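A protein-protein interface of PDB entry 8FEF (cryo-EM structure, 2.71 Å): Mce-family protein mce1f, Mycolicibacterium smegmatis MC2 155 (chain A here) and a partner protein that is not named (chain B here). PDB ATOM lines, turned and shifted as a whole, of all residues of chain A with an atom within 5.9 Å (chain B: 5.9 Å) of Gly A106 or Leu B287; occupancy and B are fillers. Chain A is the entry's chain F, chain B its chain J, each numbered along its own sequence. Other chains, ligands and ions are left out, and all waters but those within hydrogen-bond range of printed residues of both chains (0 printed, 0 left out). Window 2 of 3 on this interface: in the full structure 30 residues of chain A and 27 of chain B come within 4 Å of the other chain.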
ATOM      1  N   TYR A  54      24.121   5.012  -4.262  1.00  0.00           N
ATOM      2  CA  TYR A  54      25.088   4.076  -4.811  1.00  0.00           C
ATOM      3  C   TYR A  54      26.414   4.232  -4.082  1.00  0.00           C
ATOM      4  O   TYR A  54      26.637   5.207  -3.364  1.00  0.00           O
ATOM      5  CB  TYR A  54      25.274   4.291  -6.322  1.00  0.00           C
ATOM      6  CG  TYR A  54      25.430   5.744  -6.728  1.00  0.00           C
ATOM      7  CD1 TYR A  54      26.658   6.382  -6.650  1.00  0.00           C
ATOM      8  CD2 TYR A  54      24.347   6.473  -7.198  1.00  0.00           C
ATOM      9  CE1 TYR A  54      26.803   7.701  -7.017  1.00  0.00           C
ATOM     10  CE2 TYR A  54      24.483   7.796  -7.569  1.00  0.00           C
ATOM     11  CZ  TYR A  54      25.714   8.404  -7.477  1.00  0.00           C
ATOM     12  OH  TYR A  54      25.858   9.720  -7.847  1.00  0.00           O
ATOM     13  N   SER A 101      18.830  13.982  -3.971  1.00  0.00           N
ATOM     14  CA  SER A 101      19.302  14.104  -5.343  1.00  0.00           C
ATOM     15  C   SER A 101      19.602  15.569  -5.624  1.00  0.00           C
ATOM     16  O   SER A 101      18.796  16.443  -5.288  1.00  0.00           O
ATOM     17  CB  SER A 101      18.261  13.566  -6.328  1.00  0.00           C
ATOM     18  OG  SER A 101      18.761  13.565  -7.650  1.00  0.00           O
ATOM     19  N   VAL A 102      20.766  15.835  -6.218  1.00  0.00           N
ATOM     20  CA  VAL A 102      21.213  17.212  -6.410  1.00  0.00           C
ATOM     21  C   VAL A 102      20.300  17.945  -7.387  1.00  0.00           C
ATOM     22  O   VAL A 102      19.883  19.083  -7.141  1.00  0.00           O
ATOM     23  CB  VAL A 102      22.679  17.243  -6.875  1.00  0.00           C
ATOM     24  CG1 VAL A 102      23.102  18.660  -7.208  1.00  0.00           C
ATOM     25  CG2 VAL A 102      23.581  16.667  -5.804  1.00  0.00           C
ATOM     26  N   SER A 103      19.970  17.304  -8.506  1.00  0.00           N
ATOM     27  CA  SER A 103      19.165  17.924  -9.546  1.00  0.00           C
ATOM     28  C   SER A 103      18.262  16.866 -10.163  1.00  0.00           C
ATOM     29  O   SER A 103      18.257  15.704  -9.747  1.00  0.00           O
ATOM     30  CB  SER A 103      20.045  18.589 -10.609  1.00  0.00           C
ATOM     31  OG  SER A 103      20.880  17.642 -11.250  1.00  0.00           O
ATOM     32  N   ALA A 104      17.487  17.278 -11.167  1.00  0.00           N
ATOM     33  CA  ALA A 104      16.578  16.356 -11.833  1.00  0.00           C
ATOM     34  C   ALA A 104      17.317  15.325 -12.672  1.00  0.00           C
ATOM     35  O   ALA A 104      16.737  14.287 -13.006  1.00  0.00           O
ATOM     36  CB  ALA A 104      15.593  17.129 -12.707  1.00  0.00           C
ATOM     37  N   VAL A 105      18.572  15.595 -13.032  1.00  0.00           N
ATOM     38  CA  VAL A 105      19.353  14.634 -13.803  1.00  0.00           C
ATOM     39  C   VAL A 105      19.746  13.439 -12.939  1.00  0.00           C
ATOM     40  O   VAL A 105      19.645  12.285 -13.372  1.00  0.00           O
ATOM     41  CB  VAL A 105      20.584  15.325 -14.416  1.00  0.00           C
ATOM     42  CG1 VAL A 105      21.367  14.351 -15.270  1.00  0.00           C
ATOM     43  CG2 VAL A 105      20.156  16.525 -15.238  1.00  0.00           C
ATOM     44  N   GLY A 106      20.198  13.691 -11.712  1.00  0.00           N
ATOM     45  CA  GLY A 106      20.612  12.621 -10.823  1.00  0.00           C
ATOM     46  C   GLY A 106      21.572  13.068  -9.738  1.00  0.00           C
ATOM     47  O   GLY A 106      21.284  14.020  -9.008  1.00  0.00           O
ATOM     48  N   GLU A 107      22.713  12.380  -9.626  1.00  0.00           N
ATOM     49  CA  GLU A 107      23.759  12.663  -8.639  1.00  0.00           C
ATOM     50  C   GLU A 107      23.223  12.552  -7.206  1.00  0.00           C
ATOM     51  O   GLU A 107      23.106  13.530  -6.468  1.00  0.00           O
ATOM     52  CB  GLU A 107      24.396  14.036  -8.885  1.00  0.00           C
ATOM     53  CG  GLU A 107      25.721  14.238  -8.169  1.00  0.00           C
ATOM     54  CD  GLU A 107      26.296  15.619  -8.389  1.00  0.00           C
ATOM     55  OE1 GLU A 107      25.859  16.300  -9.339  1.00  0.00           O
ATOM     56  OE2 GLU A 107      27.180  16.027  -7.607  1.00  0.00           O
ATOM     57  N   GLN A 108      22.873  11.321  -6.845  1.00  0.00           N
ATOM     58  CA  GLN A 108      22.397  11.036  -5.501  1.00  0.00           C
ATOM     59  C   GLN A 108      23.507  11.239  -4.471  1.00  0.00           C
ATOM     60  O   GLN A 108      24.700  11.159  -4.775  1.00  0.00           O
ATOM     61  CB  GLN A 108      21.873   9.605  -5.410  1.00  0.00           C
ATOM     62  CG  GLN A 108      20.985   9.204  -6.563  1.00  0.00           C
ATOM     63  CD  GLN A 108      19.651   9.902  -6.518  1.00  0.00           C
ATOM     64  OE1 GLN A 108      19.278  10.614  -7.450  1.00  0.00           O
ATOM     65  NE2 GLN A 108      18.915   9.702  -5.433  1.00  0.00           N
ATOM     66  N   PHE B 108      29.136  19.729 -16.179  1.00  0.00           N
ATOM     67  CA  PHE B 108      29.576  18.343 -16.228  1.00  0.00           C
ATOM     68  C   PHE B 108      30.932  18.171 -16.899  1.00  0.00           C
ATOM     69  O   PHE B 108      31.382  17.030 -17.055  1.00  0.00           O
ATOM     70  CB  PHE B 108      28.540  17.485 -16.961  1.00  0.00           C
ATOM     71  CG  PHE B 108      27.261  17.290 -16.200  1.00  0.00           C
ATOM     72  CD1 PHE B 108      27.221  17.445 -14.826  1.00  0.00           C
ATOM     73  CD2 PHE B 108      26.097  16.937 -16.862  1.00  0.00           C
ATOM     74  CE1 PHE B 108      26.045  17.259 -14.129  1.00  0.00           C
ATOM     75  CE2 PHE B 108      24.919  16.750 -16.169  1.00  0.00           C
ATOM     76  CZ  PHE B 108      24.895  16.912 -14.801  1.00  0.00           C
ATOM     77  N   PHE B 214      33.143  11.702  -9.784  1.00  0.00           N
ATOM     78  CA  PHE B 214      32.865  10.715 -10.818  1.00  0.00           C
ATOM     79  C   PHE B 214      34.120  10.031 -11.343  1.00  0.00           C
ATOM     80  O   PHE B 214      34.060   9.363 -12.381  1.00  0.00           O
ATOM     81  CB  PHE B 214      32.095  11.366 -11.967  1.00  0.00           C
ATOM     82  CG  PHE B 214      30.746  11.891 -11.566  1.00  0.00           C
ATOM     83  CD1 PHE B 214      30.604  13.183 -11.093  1.00  0.00           C
ATOM     84  CD2 PHE B 214      29.624  11.089 -11.655  1.00  0.00           C
ATOM     85  CE1 PHE B 214      29.367  13.664 -10.718  1.00  0.00           C
ATOM     86  CE2 PHE B 214      28.384  11.566 -11.282  1.00  0.00           C
ATOM     87  CZ  PHE B 214      28.256  12.855 -10.815  1.00  0.00           C
ATOM     88  N   PHE B 285      30.059   3.282 -13.264  1.00  0.00           N
ATOM     89  CA  PHE B 285      29.688   4.693 -13.283  1.00  0.00           C
ATOM     90  C   PHE B 285      28.203   4.811 -12.979  1.00  0.00           C
ATOM     91  O   PHE B 285      27.383   4.165 -13.640  1.00  0.00           O
ATOM     92  CB  PHE B 285      30.014   5.335 -14.638  1.00  0.00           C
ATOM     93  CG  PHE B 285      29.284   6.620 -14.892  1.00  0.00           C
ATOM     94  CD1 PHE B 285      29.591   7.760 -14.172  1.00  0.00           C
ATOM     95  CD2 PHE B 285      28.292   6.689 -15.855  1.00  0.00           C
ATOM     96  CE1 PHE B 285      28.918   8.941 -14.402  1.00  0.00           C
ATOM     97  CE2 PHE B 285      27.617   7.868 -16.091  1.00  0.00           C
ATOM     98  CZ  PHE B 285      27.929   8.995 -15.364  1.00  0.00           C
ATOM     99  N   ASN B 286      27.860   5.631 -11.986  1.00  0.00           N
ATOM    100  CA  ASN B 286      26.480   5.824 -11.561  1.00  0.00           C
ATOM    101  C   ASN B 286      26.167   7.311 -11.485  1.00  0.00           C
ATOM    102  O   ASN B 286      26.915   8.072 -10.865  1.00  0.00           O
ATOM    103  CB  ASN B 286      26.220   5.176 -10.197  1.00  0.00           C
ATOM    104  CG  ASN B 286      26.415   3.678 -10.214  1.00  0.00           C
ATOM    105  OD1 ASN B 286      27.524   3.182 -10.025  1.00  0.00           O
ATOM    106  ND2 ASN B 286      25.332   2.944 -10.437  1.00  0.00           N
ATOM    107  N   LEU B 287      25.075   7.722 -12.126  1.00  0.00           N
ATOM    108  CA  LEU B 287      24.538   9.067 -11.965  1.00  0.00           C
ATOM    109  C   LEU B 287      23.098   9.068 -11.477  1.00  0.00           C
ATOM    110  O   LEU B 287      22.768   9.789 -10.528  1.00  0.00           O
ATOM    111  CB  LEU B 287      24.641   9.844 -13.284  1.00  0.00           C
ATOM    112  CG  LEU B 287      24.092  11.270 -13.237  1.00  0.00           C
ATOM    113  CD1 LEU B 287      24.988  12.166 -12.400  1.00  0.00           C
ATOM    114  CD2 LEU B 287      23.941  11.820 -14.634  1.00  0.00           C
ATOM    115  N   THR B 288      22.230   8.277 -12.100  1.00  0.00           N
ATOM    116  CA  THR B 288      20.805   8.282 -11.808  1.00  0.00           C
ATOM    117  C   THR B 288      20.515   7.341 -10.638  1.00  0.00           C
ATOM    118  O   THR B 288      21.425   6.781 -10.023  1.00  0.00           O
ATOM    119  CB  THR B 288      20.008   7.903 -13.055  1.00  0.00           C
ATOM    120  OG1 THR B 288      18.607   7.930 -12.756  1.00  0.00           O
ATOM    121  CG2 THR B 288      20.389   6.510 -13.524  1.00  0.00           C
ATOM    122  N   VAL B 289      19.238   7.156 -10.321  1.00  0.00           N
ATOM    123  CA  VAL B 289      18.859   6.299  -9.205  1.00  0.00           C
ATOM    124  C   VAL B 289      18.980   4.837  -9.617  1.00  0.00           C
ATOM    125  O   VAL B 289      18.866   3.932  -8.791  1.00  0.00           O
ATOM    126  CB  VAL B 289      17.426   6.599  -8.708  1.00  0.00           C
ATOM    127  CG1 VAL B 289      17.325   8.010  -8.156  1.00  0.00           C
ATOM    128  CG2 VAL B 289      16.416   6.361  -9.791  1.00  0.00           C
ATOM    129  OXT VAL B 289      19.193   4.521 -10.788  1.00  0.00           O
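The backbone carbonyl oxygen (O) of Leu B287 sits at hydrogen-bond distance from the backbone NH (N) of Glu A107 (2.7 Å).
OG of Ser A101 sits at hydrogen-bond distance from OE1 of Gln A108, at 3.0 Å. OG of Ser A101 is in hydrogen-bond range of O of Gly A106. The backbone NH of Val A102 sits close to the backbone carbonyl oxygen of Glu A107 (3.3 Å).
Tyr A54 touches Asn B286 (OH to O, 3.6 Å). O of Leu B287 touches CE2 of Tyr A54, 3.96 Å away. CG1 of Val A105 touches CD2 of Leu B287, 3.7 Å away. Gly A106 touches Leu B287 (CA to O, 3.6 Å). Phe B214 touches Glu A107 (CZ to CG, 3.9 Å). O of Leu B287 touches N of Gln A108, at 3.99 Å. Val B289 touches Gln A108.
Of the printed residues of chain B, Val A105 touches Leu B287. Gly A106 touches just one residue of chain B: Leu B287 (3.6 Å). Printed residues of chain B within 4 Å of Glu A107: Phe B214 and Leu B287. Printed residues of chain B within 4 Å of Gln A108: Leu B287 (3.99 Å) and Val B289 (3.3 Å). Printed residues of chain A within 4 Å of Val B289: Gln A108.
Of the 9 printed residues of chain A, 5 touch a printed residue of chain B. Hydrophobic or aromatic side chains of chain A that line the printed part of chain B: Tyr A54 and Val A105. Of the 7 printed residues of chain B, 4 touch a printed residue of chain A. Printed residues of chain B that touch a printed residue of chain A: Phe B214, Asn B286, Leu B287 and Val B289. Among the printed residues, 8 pairs touch across the chains.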
